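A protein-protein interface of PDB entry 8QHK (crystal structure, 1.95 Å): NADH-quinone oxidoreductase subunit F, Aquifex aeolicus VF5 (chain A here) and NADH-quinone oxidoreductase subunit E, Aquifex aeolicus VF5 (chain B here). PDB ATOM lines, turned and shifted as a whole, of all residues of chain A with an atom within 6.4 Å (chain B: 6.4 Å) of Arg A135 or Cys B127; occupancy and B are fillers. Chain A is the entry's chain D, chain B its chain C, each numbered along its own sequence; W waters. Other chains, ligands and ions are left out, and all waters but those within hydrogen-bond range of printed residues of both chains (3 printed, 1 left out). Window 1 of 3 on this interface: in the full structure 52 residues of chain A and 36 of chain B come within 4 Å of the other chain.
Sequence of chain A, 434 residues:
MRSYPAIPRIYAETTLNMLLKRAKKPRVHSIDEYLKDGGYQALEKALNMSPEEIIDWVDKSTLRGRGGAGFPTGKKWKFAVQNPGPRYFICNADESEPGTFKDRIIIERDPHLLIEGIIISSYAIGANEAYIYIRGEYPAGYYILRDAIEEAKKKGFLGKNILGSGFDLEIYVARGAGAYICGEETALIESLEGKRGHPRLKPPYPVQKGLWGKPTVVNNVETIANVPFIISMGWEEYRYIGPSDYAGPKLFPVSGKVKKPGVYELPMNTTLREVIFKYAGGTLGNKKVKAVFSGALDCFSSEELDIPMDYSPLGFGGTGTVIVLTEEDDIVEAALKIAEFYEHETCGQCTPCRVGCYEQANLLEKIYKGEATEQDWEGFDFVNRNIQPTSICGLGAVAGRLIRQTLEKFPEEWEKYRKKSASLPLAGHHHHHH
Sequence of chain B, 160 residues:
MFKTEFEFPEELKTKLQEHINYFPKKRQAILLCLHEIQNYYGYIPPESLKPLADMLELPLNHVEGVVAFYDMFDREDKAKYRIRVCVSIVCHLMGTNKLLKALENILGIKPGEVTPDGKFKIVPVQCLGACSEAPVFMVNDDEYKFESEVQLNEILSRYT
SG of Cys B131 lies close to N of Gly A99, 3.3 Å away. The guanidinium group (NH2) of Arg A135 lies within hydrogen-bond range of the backbone carbonyl oxygen (O) of Cys B127. The backbone carbonyl oxygen (O) of Ala A177 sits at hydrogen-bond distance from the backbone NH (N) of Met B72, 2.9 Å away. The side-chain sulfur of Cys B127 lies close to the backbone NH of Gly A99 (3.8 Å).
O of Glu A95 is in hydrogen-bond range of NH1 of Arg A135 (2.8 Å). The guanidinium group (NE) of Arg A135 sits close to the side-chain hydroxyl (OG) of Ser A96. OE1 of Glu A95 is in hydrogen-bond range of OH of Tyr A138 (2.7 Å). The side-chain hydroxyl (OG) of Ser B88 sits at hydrogen-bond distance from the backbone NH (N) of Cys B127 (2.9 Å). The side-chain amide oxygen (OE1) of Gln B126 is in hydrogen-bond range of the side-chain hydroxyl (OG) of Ser B88, at 3.2 Å. The backbone NH (N) of Gly A136 lies close to the backbone carbonyl oxygen (O) of Gly A176, at 3.5 Å.
Among the printed residues, pairs that only touch across the chains: Gly A136 with Met B72, Arg A135 with Leu B128, Tyr A138 with Leu B128, Phe A341 with Gln B126, Arg A135 with Gly B129, Thr A100 with Gly B129, Tyr A138 with Gly B129, Pro A98 with Cys B127, Gly A178 with Met B72, Glu A137 with Met B72, Pro A98 with Ile B89 and Thr A100 with Cys B131.
Printed residues of chain A within 4 Å of Cys B127: Pro A98 (3.7 Å), Gly A99 (3.8 Å) and Arg A135 (2.7 Å). Of the printed residues of chain A, Leu B128 touches Arg A135 and Tyr A138. Of the printed residues of chain A, Cys B131 touches Gly A99 (3.3 Å) and Thr A100 (3.9 Å). Printed residues of chain B within 4 Å of Glu A137: Met B72. Of the printed residues of chain B, Ala A177 touches Met B72. Ser B88 touches none of the printed residues of chain A. The nearest printed residue of chain A that does not touch Cys B127 is Glu A97 (4.01 Å). The nearest printed residue of chain B that does not touch Thr A100 is Cys B127 (4.8 Å).
Hydrophobic or aromatic side chains of chain A within 4 Å of the printed part of chain B: Pro A98, Tyr A138 and Phe A341. Among the printed residues, 16 pairs touch across the chains.
Water W3 bridges the backbone carbonyl oxygen (O) of Leu B128 (2.5 Å) and the backbone carbonyl oxygen (O) of Glu A137 (2.8 Å). Water W2 bridges the backbone carbonyl oxygen (O) of Ser A96 (2.8 Å) and the backbone carbonyl oxygen (O) of Cys B127 (2.8 Å). Water W1 lies within hydrogen-bond range of O of Gln B126 (2.9 Å), NH2 of Arg A135 (3.4 Å) and OE2 of Glu A137 (3.5 Å).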
ATOM      1  N   ALA A  93      21.723  14.637 -12.793  1.00  0.00           N
ATOM      2  CA  ALA A  93      22.239  13.529 -11.995  1.00  0.00           C
ATOM      3  C   ALA A  93      22.634  12.350 -12.888  1.00  0.00           C
ATOM      4  O   ALA A  93      22.479  11.188 -12.493  1.00  0.00           O
ATOM      5  CB  ALA A  93      21.188  13.108 -10.984  1.00  0.00           C
ATOM      6  N   ASP A  94      23.146  12.648 -14.096  1.00  0.00           N
ATOM      7  CA  ASP A  94      23.518  11.600 -15.035  1.00  0.00           C
ATOM      8  C   ASP A  94      24.911  11.035 -14.744  1.00  0.00           C
ATOM      9  O   ASP A  94      25.229   9.973 -15.279  1.00  0.00           O
ATOM     10  CB  ASP A  94      23.440  12.045 -16.499  1.00  0.00           C
ATOM     11  CG  ASP A  94      23.310  10.847 -17.428  1.00  0.00           C
ATOM     12  OD1 ASP A  94      22.330  10.090 -17.256  1.00  0.00           O
ATOM     13  OD2 ASP A  94      24.213  10.643 -18.272  1.00  0.00           O
ATOM     14  N   GLU A  95      25.710  11.742 -13.918  1.00  0.00           N
ATOM     15  CA  GLU A  95      27.066  11.384 -13.499  1.00  0.00           C
ATOM     16  C   GLU A  95      27.550  10.043 -14.052  1.00  0.00           C
ATOM     17  O   GLU A  95      27.295   9.002 -13.456  1.00  0.00           O
ATOM     18  CB  GLU A  95      27.135  11.320 -11.973  1.00  0.00           C
ATOM     19  CG  GLU A  95      28.503  10.927 -11.438  1.00  0.00           C
ATOM     20  CD  GLU A  95      28.645  11.124  -9.938  1.00  0.00           C
ATOM     21  OE1 GLU A  95      27.961  10.394  -9.194  1.00  0.00           O
ATOM     22  OE2 GLU A  95      29.406  12.038  -9.528  1.00  0.00           O
ATOM     23  N   SER A  96      28.306  10.074 -15.155  1.00  0.00           N
ATOM     24  CA  SER A  96      28.775   8.858 -15.811  1.00  0.00           C
ATOM     25  C   SER A  96      30.221   8.977 -16.289  1.00  0.00           C
ATOM     26  O   SER A  96      30.717   8.071 -16.947  1.00  0.00           O
ATOM     27  CB  SER A  96      27.871   8.499 -16.976  1.00  0.00           C
ATOM     28  OG  SER A  96      26.614   8.047 -16.505  1.00  0.00           O
ATOM     29  N   GLU A  97      30.890  10.090 -15.986  1.00  0.00           N
ATOM     30  CA  GLU A  97      32.309  10.226 -16.287  1.00  0.00           C
ATOM     31  C   GLU A  97      33.104   9.170 -15.524  1.00  0.00           C
ATOM     32  O   GLU A  97      32.916   9.041 -14.317  1.00  0.00           O
ATOM     33  CB  GLU A  97      32.787  11.609 -15.848  1.00  0.00           C
ATOM     34  CG  GLU A  97      34.237  11.899 -16.170  1.00  0.00           C
ATOM     35  CD  GLU A  97      34.530  12.263 -17.611  1.00  0.00           C
ATOM     36  OE1 GLU A  97      33.635  12.053 -18.474  1.00  0.00           O
ATOM     37  OE2 GLU A  97      35.642  12.793 -17.861  1.00  0.00           O
ATOM     38  N   PRO A  98      34.045   8.428 -16.156  1.00  0.00           N
ATOM     39  CA  PRO A  98      34.965   7.557 -15.424  1.00  0.00           C
ATOM     40  C   PRO A  98      35.612   8.212 -14.207  1.00  0.00           C
ATOM     41  O   PRO A  98      36.074   9.353 -14.273  1.00  0.00           O
ATOM     42  CB  PRO A  98      36.035   7.231 -16.469  1.00  0.00           C
ATOM     43  CG  PRO A  98      35.242   7.189 -17.750  1.00  0.00           C
ATOM     44  CD  PRO A  98      34.268   8.342 -17.608  1.00  0.00           C
ATOM     45  N   GLY A  99      35.609   7.468 -13.098  1.00  0.00           N
ATOM     46  CA  GLY A  99      36.195   7.915 -11.847  1.00  0.00           C
ATOM     47  C   GLY A  99      35.257   8.791 -11.021  1.00  0.00           C
ATOM     48  O   GLY A  99      35.607   9.188  -9.908  1.00  0.00           O
ATOM     49  N   THR A 100      34.067   9.097 -11.549  1.00  0.00           N
ATOM     50  CA  THR A 100      33.259  10.153 -10.947  1.00  0.00           C
ATOM     51  C   THR A 100      32.058   9.546 -10.223  1.00  0.00           C
ATOM     52  O   THR A 100      31.209   8.918 -10.844  1.00  0.00           O
ATOM     53  CB  THR A 100      32.885  11.224 -11.986  1.00  0.00           C
ATOM     54  OG1 THR A 100      34.076  11.531 -12.718  1.00  0.00           O
ATOM     55  CG2 THR A 100      32.308  12.473 -11.355  1.00  0.00           C
ATOM     56  N   TYR A 133      17.163  14.319 -13.636  1.00  0.00           N
ATOM     57  CA  TYR A 133      17.482  13.259 -14.576  1.00  0.00           C
ATOM     58  C   TYR A 133      18.625  12.442 -13.988  1.00  0.00           C
ATOM     59  O   TYR A 133      19.742  12.946 -13.889  1.00  0.00           O
ATOM     60  CB  TYR A 133      17.839  13.854 -15.938  1.00  0.00           C
ATOM     61  CG  TYR A 133      17.976  12.841 -17.045  1.00  0.00           C
ATOM     62  CD1 TYR A 133      19.130  12.090 -17.203  1.00  0.00           C
ATOM     63  CD2 TYR A 133      16.937  12.610 -17.926  1.00  0.00           C
ATOM     64  CE1 TYR A 133      19.262  11.176 -18.235  1.00  0.00           C
ATOM     65  CE2 TYR A 133      17.048  11.691 -18.955  1.00  0.00           C
ATOM     66  CZ  TYR A 133      18.211  10.964 -19.106  1.00  0.00           C
ATOM     67  OH  TYR A 133      18.289  10.047 -20.126  1.00  0.00           O
ATOM     68  N   ILE A 134      18.318  11.224 -13.527  1.00  0.00           N
ATOM     69  CA  ILE A 134      19.307  10.362 -12.901  1.00  0.00           C
ATOM     70  C   ILE A 134      19.601   9.182 -13.822  1.00  0.00           C
ATOM     71  O   ILE A 134      18.691   8.526 -14.351  1.00  0.00           O
ATOM     72  CB  ILE A 134      18.877   9.925 -11.483  1.00  0.00           C
ATOM     73  CG1 ILE A 134      20.000   9.181 -10.754  1.00  0.00           C
ATOM     74  CG2 ILE A 134      17.598   9.104 -11.494  1.00  0.00           C
ATOM     75  CD1 ILE A 134      19.733   8.948  -9.286  1.00  0.00           C
ATOM     76  N   ARG A 135      20.899   8.909 -14.011  1.00  0.00           N
ATOM     77  CA  ARG A 135      21.297   7.812 -14.873  1.00  0.00           C
ATOM     78  C   ARG A 135      20.578   6.544 -14.420  1.00  0.00           C
ATOM     79  O   ARG A 135      20.255   6.386 -13.244  1.00  0.00           O
ATOM     80  CB  ARG A 135      22.813   7.612 -14.844  1.00  0.00           C
ATOM     81  CG  ARG A 135      23.352   7.170 -13.487  1.00  0.00           C
ATOM     82  CD  ARG A 135      24.862   7.051 -13.478  1.00  0.00           C
ATOM     83  NE  ARG A 135      25.330   5.971 -14.328  1.00  0.00           N
ATOM     84  CZ  ARG A 135      26.595   5.566 -14.402  1.00  0.00           C
ATOM     85  NH1 ARG A 135      27.533   6.178 -13.696  1.00  0.00           N
ATOM     86  NH2 ARG A 135      26.914   4.551 -15.190  1.00  0.00           N
ATOM     87  N   GLY A 136      20.348   5.647 -15.377  1.00  0.00           N
ATOM     88  CA  GLY A 136      19.614   4.420 -15.140  1.00  0.00           C
ATOM     89  C   GLY A 136      20.369   3.429 -14.263  1.00  0.00           C
ATOM     90  O   GLY A 136      19.742   2.543 -13.687  1.00  0.00           O
ATOM     91  N   GLU A 137      21.700   3.570 -14.181  1.00  0.00           N
ATOM     92  CA  GLU A 137      22.541   2.660 -13.408  1.00  0.00           C
ATOM     93  C   GLU A 137      22.631   3.085 -11.935  1.00  0.00           C
ATOM     94  O   GLU A 137      23.383   2.479 -11.165  1.00  0.00           O
ATOM     95  CB  GLU A 137      23.945   2.567 -14.014  1.00  0.00           C
ATOM     96  CG  GLU A 137      23.989   2.107 -15.469  1.00  0.00           C
ATOM     97  CD  GLU A 137      23.799   3.204 -16.515  1.00  0.00           C
ATOM     98  OE1 GLU A 137      23.548   4.379 -16.122  1.00  0.00           O
ATOM     99  OE2 GLU A 137      23.901   2.885 -17.731  1.00  0.00           O
ATOM    100  N   TYR A 138      21.859   4.116 -11.545  1.00  0.00           N
ATOM    101  CA  TYR A 138      21.673   4.492 -10.149  1.00  0.00           C
ATOM    102  C   TYR A 138      20.235   4.190  -9.713  1.00  0.00           C
ATOM    103  O   TYR A 138      19.484   5.106  -9.361  1.00  0.00           O
ATOM    104  CB  TYR A 138      21.953   5.988  -9.931  1.00  0.00           C
ATOM    105  CG  TYR A 138      23.391   6.463  -9.976  1.00  0.00           C
ATOM    106  CD1 TYR A 138      24.474   5.593  -9.972  1.00  0.00           C
ATOM    107  CD2 TYR A 138      23.670   7.819 -10.005  1.00  0.00           C
ATOM    108  CE1 TYR A 138      25.780   6.058  -9.984  1.00  0.00           C
ATOM    109  CE2 TYR A 138      24.971   8.305 -10.020  1.00  0.00           C
ATOM    110  CZ  TYR A 138      26.036   7.415  -9.997  1.00  0.00           C
ATOM    111  OH  TYR A 138      27.334   7.885 -10.044  1.00  0.00           O
ATOM    112  N   PRO A 139      19.799   2.908  -9.697  1.00  0.00           N
ATOM    113  CA  PRO A 139      18.421   2.583  -9.355  1.00  0.00           C
ATOM    114  C   PRO A 139      18.077   2.933  -7.911  1.00  0.00           C
ATOM    115  O   PRO A 139      16.999   3.453  -7.645  1.00  0.00           O
ATOM    116  CB  PRO A 139      18.317   1.073  -9.607  1.00  0.00           C
ATOM    117  CG  PRO A 139      19.737   0.558  -9.530  1.00  0.00           C
ATOM    118  CD  PRO A 139      20.600   1.707  -9.987  1.00  0.00           C
ATOM    119  N   TYR A 142      17.377   6.533  -7.548  1.00  0.00           N
ATOM    120  CA  TYR A 142      16.076   6.876  -8.096  1.00  0.00           C
ATOM    121  C   TYR A 142      14.992   6.647  -7.038  1.00  0.00           C
ATOM    122  O   TYR A 142      14.164   7.517  -6.808  1.00  0.00           O
ATOM    123  CB  TYR A 142      15.803   6.088  -9.381  1.00  0.00           C
ATOM    124  CG  TYR A 142      14.373   6.158  -9.844  1.00  0.00           C
ATOM    125  CD1 TYR A 142      13.885   7.260 -10.529  1.00  0.00           C
ATOM    126  CD2 TYR A 142      13.493   5.131  -9.566  1.00  0.00           C
ATOM    127  CE1 TYR A 142      12.567   7.322 -10.957  1.00  0.00           C
ATOM    128  CE2 TYR A 142      12.171   5.179  -9.978  1.00  0.00           C
ATOM    129  CZ  TYR A 142      11.700   6.286 -10.655  1.00  0.00           C
ATOM    130  OH  TYR A 142      10.381   6.323 -11.041  1.00  0.00           O
ATOM    131  N   ALA A 174      13.257  11.656 -13.658  1.00  0.00           N
ATOM    132  CA  ALA A 174      13.385  10.882 -14.886  1.00  0.00           C
ATOM    133  C   ALA A 174      14.596   9.961 -14.762  1.00  0.00           C
ATOM    134  O   ALA A 174      15.527  10.286 -14.029  1.00  0.00           O
ATOM    135  CB  ALA A 174      13.516  11.816 -16.077  1.00  0.00           C
ATOM    136  N   ARG A 175      14.559   8.815 -15.468  1.00  0.00           N
ATOM    137  CA  ARG A 175      15.680   7.883 -15.480  1.00  0.00           C
ATOM    138  C   ARG A 175      16.301   7.831 -16.877  1.00  0.00           C
ATOM    139  O   ARG A 175      15.586   7.807 -17.878  1.00  0.00           O
ATOM    140  CB  ARG A 175      15.268   6.463 -15.082  1.00  0.00           C
ATOM    141  CG  ARG A 175      14.894   6.284 -13.621  1.00  0.00           C
ATOM    142  CD  ARG A 175      14.569   4.838 -13.293  1.00  0.00           C
ATOM    143  NE  ARG A 175      15.746   3.996 -13.109  1.00  0.00           N
ATOM    144  CZ  ARG A 175      15.719   2.665 -13.067  1.00  0.00           C
ATOM    145  NH1 ARG A 175      14.572   2.012 -13.201  1.00  0.00           N
ATOM    146  NH2 ARG A 175      16.848   1.990 -12.905  1.00  0.00           N
ATOM    147  N   GLY A 176      17.641   7.854 -16.913  1.00  0.00           N
ATOM    148  CA  GLY A 176      18.417   7.488 -18.082  1.00  0.00           C
ATOM    149  C   GLY A 176      18.335   5.992 -18.354  1.00  0.00           C
ATOM    150  O   GLY A 176      17.699   5.260 -17.598  1.00  0.00           O
ATOM    151  N   ALA A 177      18.956   5.546 -19.454  1.00  0.00           N
ATOM    152  CA  ALA A 177      18.897   4.136 -19.818  1.00  0.00           C
ATOM    153  C   ALA A 177      20.171   3.666 -20.519  1.00  0.00           C
ATOM    154  O   ALA A 177      20.103   2.816 -21.407  1.00  0.00           O
ATOM    155  CB  ALA A 177      17.666   3.881 -20.654  1.00  0.00           C
ATOM    156  N   GLY A 178      21.330   4.199 -20.107  1.00  0.00           N
ATOM    157  CA  GLY A 178      22.613   3.610 -20.474  1.00  0.00           C
ATOM    158  C   GLY A 178      23.529   4.504 -21.312  1.00  0.00           C
ATOM    159  O   GLY A 178      24.610   4.059 -21.708  1.00  0.00           O
ATOM    160  N   PHE A 341      35.936   3.703 -23.965  1.00  0.00           N
ATOM    161  CA  PHE A 341      34.861   4.481 -23.368  1.00  0.00           C
ATOM    162  C   PHE A 341      34.206   5.401 -24.407  1.00  0.00           C
ATOM    163  O   PHE A 341      32.982   5.401 -24.548  1.00  0.00           O
ATOM    164  CB  PHE A 341      35.376   5.286 -22.168  1.00  0.00           C
ATOM    165  CG  PHE A 341      34.316   6.140 -21.519  1.00  0.00           C
ATOM    166  CD1 PHE A 341      33.374   5.577 -20.668  1.00  0.00           C
ATOM    167  CD2 PHE A 341      34.221   7.492 -21.803  1.00  0.00           C
ATOM    168  CE1 PHE A 341      32.372   6.351 -20.105  1.00  0.00           C
ATOM    169  CE2 PHE A 341      33.219   8.264 -21.239  1.00  0.00           C
ATOM    170  CZ  PHE A 341      32.293   7.691 -20.401  1.00  0.00           C
ATOM    171  N   MET B  72      20.913   0.049 -21.956  1.00  0.00           N
ATOM    172  CA  MET B  72      20.434  -0.800 -20.873  1.00  0.00           C
ATOM    173  C   MET B  72      19.353  -1.776 -21.363  1.00  0.00           C
ATOM    174  O   MET B  72      19.139  -2.814 -20.737  1.00  0.00           O
ATOM    175  CB  MET B  72      19.879   0.022 -19.710  1.00  0.00           C
ATOM    176  CG  MET B  72      20.961   0.604 -18.823  1.00  0.00           C
ATOM    177  SD  MET B  72      20.278   1.501 -17.399  1.00  0.00           S
ATOM    178  CE  MET B  72      20.007   0.153 -16.250  1.00  0.00           C
ATOM    179  N   CYS B  86      31.495  -3.761 -14.717  1.00  0.00           N
ATOM    180  CA  CYS B  86      32.163  -2.574 -15.224  1.00  0.00           C
ATOM    181  C   CYS B  86      33.521  -2.925 -15.830  1.00  0.00           C
ATOM    182  O   CYS B  86      34.353  -3.574 -15.192  1.00  0.00           O
ATOM    183  CB  CYS B  86      32.362  -1.536 -14.135  1.00  0.00           C
ATOM    184  SG  CYS B  86      33.293  -0.105 -14.732  1.00  0.00           S
ATOM    185  N   VAL B  87      33.745  -2.448 -17.059  1.00  0.00           N
ATOM    186  CA  VAL B  87      34.972  -2.729 -17.786  1.00  0.00           C
ATOM    187  C   VAL B  87      35.741  -1.439 -18.075  1.00  0.00           C
ATOM    188  O   VAL B  87      36.646  -1.447 -18.901  1.00  0.00           O
ATOM    189  CB  VAL B  87      34.679  -3.528 -19.074  1.00  0.00           C
ATOM    190  CG1 VAL B  87      34.028  -4.868 -18.757  1.00  0.00           C
ATOM    191  CG2 VAL B  87      33.831  -2.750 -20.075  1.00  0.00           C
ATOM    192  N   SER B  88      35.421  -0.342 -17.380  1.00  0.00           N
ATOM    193  CA  SER B  88      36.101   0.929 -17.606  1.00  0.00           C
ATOM    194  C   SER B  88      37.392   0.994 -16.797  1.00  0.00           C
ATOM    195  O   SER B  88      37.723   0.056 -16.074  1.00  0.00           O
ATOM    196  CB  SER B  88      35.200   2.097 -17.297  1.00  0.00           C
ATOM    197  OG  SER B  88      34.165   2.187 -18.248  1.00  0.00           O
ATOM    198  N   ILE B  89      38.089   2.129 -16.921  1.00  0.00           N
ATOM    199  CA  ILE B  89      39.487   2.287 -16.555  1.00  0.00           C
ATOM    200  C   ILE B  89      39.751   1.890 -15.099  1.00  0.00           C
ATOM    201  O   ILE B  89      40.710   1.160 -14.836  1.00  0.00           O
ATOM    202  CB  ILE B  89      39.977   3.721 -16.872  1.00  0.00           C
ATOM    203  CG1 ILE B  89      41.422   3.951 -16.413  1.00  0.00           C
ATOM    204  CG2 ILE B  89      39.062   4.789 -16.295  1.00  0.00           C
ATOM    205  CD1 ILE B  89      42.425   3.147 -17.168  1.00  0.00           C
ATOM    206  N   VAL B  90      38.955   2.375 -14.136  1.00  0.00           N
ATOM    207  CA  VAL B  90      39.329   2.145 -12.742  1.00  0.00           C
ATOM    208  C   VAL B  90      39.161   0.666 -12.400  1.00  0.00           C
ATOM    209  O   VAL B  90      40.096   0.032 -11.908  1.00  0.00           O
ATOM    210  CB  VAL B  90      38.600   3.044 -11.731  1.00  0.00           C
ATOM    211  CG1 VAL B  90      39.209   2.873 -10.344  1.00  0.00           C
ATOM    212  CG2 VAL B  90      38.633   4.505 -12.146  1.00  0.00           C
ATOM    213  N   VAL B 125      29.628  -3.342 -18.889  1.00  0.00           N
ATOM    214  CA  VAL B 125      29.126  -1.976 -18.927  1.00  0.00           C
ATOM    215  C   VAL B 125      30.286  -1.017 -18.683  1.00  0.00           C
ATOM    216  O   VAL B 125      31.335  -1.414 -18.188  1.00  0.00           O
ATOM    217  CB  VAL B 125      27.988  -1.757 -17.912  1.00  0.00           C
ATOM    218  CG1 VAL B 125      26.762  -2.589 -18.253  1.00  0.00           C
ATOM    219  CG2 VAL B 125      28.440  -2.032 -16.480  1.00  0.00           C
ATOM    220  N   GLN B 126      30.077   0.250 -19.043  1.00  0.00           N
ATOM    221  CA  GLN B 126      31.035   1.308 -18.768  1.00  0.00           C
ATOM    222  C   GLN B 126      30.867   1.744 -17.313  1.00  0.00           C
ATOM    223  O   GLN B 126      29.990   1.240 -16.621  1.00  0.00           O
ATOM    224  CB  GLN B 126      30.832   2.461 -19.757  1.00  0.00           C
ATOM    225  CG  GLN B 126      30.949   2.063 -21.231  1.00  0.00           C
ATOM    226  CD  GLN B 126      32.281   1.453 -21.605  1.00  0.00           C
ATOM    227  OE1 GLN B 126      33.354   1.969 -21.288  1.00  0.00           O
ATOM    228  NE2 GLN B 126      32.219   0.322 -22.290  1.00  0.00           N
ATOM    229  N   CYS B 127      31.707   2.692 -16.877  1.00  0.00           N
ATOM    230  CA  CYS B 127      31.818   3.129 -15.490  1.00  0.00           C
ATOM    231  C   CYS B 127      30.454   3.269 -14.809  1.00  0.00           C
ATOM    232  O   CYS B 127      29.588   4.014 -15.274  1.00  0.00           O
ATOM    233  CB  CYS B 127      32.568   4.454 -15.412  1.00  0.00           C
ATOM    234  SG  CYS B 127      32.753   5.075 -13.721  1.00  0.00           S
ATOM    235  N   LEU B 128      30.316   2.584 -13.665  1.00  0.00           N
ATOM    236  CA  LEU B 128      29.079   2.509 -12.901  1.00  0.00           C
ATOM    237  C   LEU B 128      29.020   3.587 -11.821  1.00  0.00           C
ATOM    238  O   LEU B 128      28.102   3.596 -11.002  1.00  0.00           O
ATOM    239  CB  LEU B 128      28.980   1.115 -12.271  1.00  0.00           C
ATOM    240  CG  LEU B 128      28.590  -0.010 -13.231  1.00  0.00           C
ATOM    241  CD1 LEU B 128      28.683  -1.367 -12.549  1.00  0.00           C
ATOM    242  CD2 LEU B 128      27.187   0.207 -13.773  1.00  0.00           C
ATOM    243  N   GLY B 129      30.031   4.451 -11.753  1.00  0.00           N
ATOM    244  CA  GLY B 129      30.032   5.497 -10.746  1.00  0.00           C
ATOM    245  C   GLY B 129      30.197   4.940  -9.334  1.00  0.00           C
ATOM    246  O   GLY B 129      29.569   5.438  -8.401  1.00  0.00           O
ATOM    247  N   ALA B 130      31.068   3.929  -9.178  1.00  0.00           N
ATOM    248  CA  ALA B 130      31.434   3.437  -7.854  1.00  0.00           C
ATOM    249  C   ALA B 130      32.915   3.071  -7.799  1.00  0.00           C
ATOM    250  O   ALA B 130      33.295   2.107  -7.136  1.00  0.00           O
ATOM    251  CB  ALA B 130      30.576   2.257  -7.492  1.00  0.00           C
ATOM    252  N   CYS B 131      33.746   3.925  -8.403  1.00  0.00           N
ATOM    253  CA  CYS B 131      35.100   3.571  -8.800  1.00  0.00           C
ATOM    254  C   CYS B 131      36.005   3.352  -7.585  1.00  0.00           C
ATOM    255  O   CYS B 131      36.974   2.598  -7.651  1.00  0.00           O
ATOM    256  CB  CYS B 131      35.674   4.646  -9.722  1.00  0.00           C
ATOM    257  SG  CYS B 131      34.480   5.243 -10.954  1.00  0.00           S
HETATM  258  O   HOH W   1      27.200   1.897 -17.235  1.00  0.00           O
HETATM  259  O   HOH W   2      29.837   5.531 -17.587  1.00  0.00           O
HETATM  260  O   HOH W   3      26.045   2.285 -10.412  1.00  0.00           O
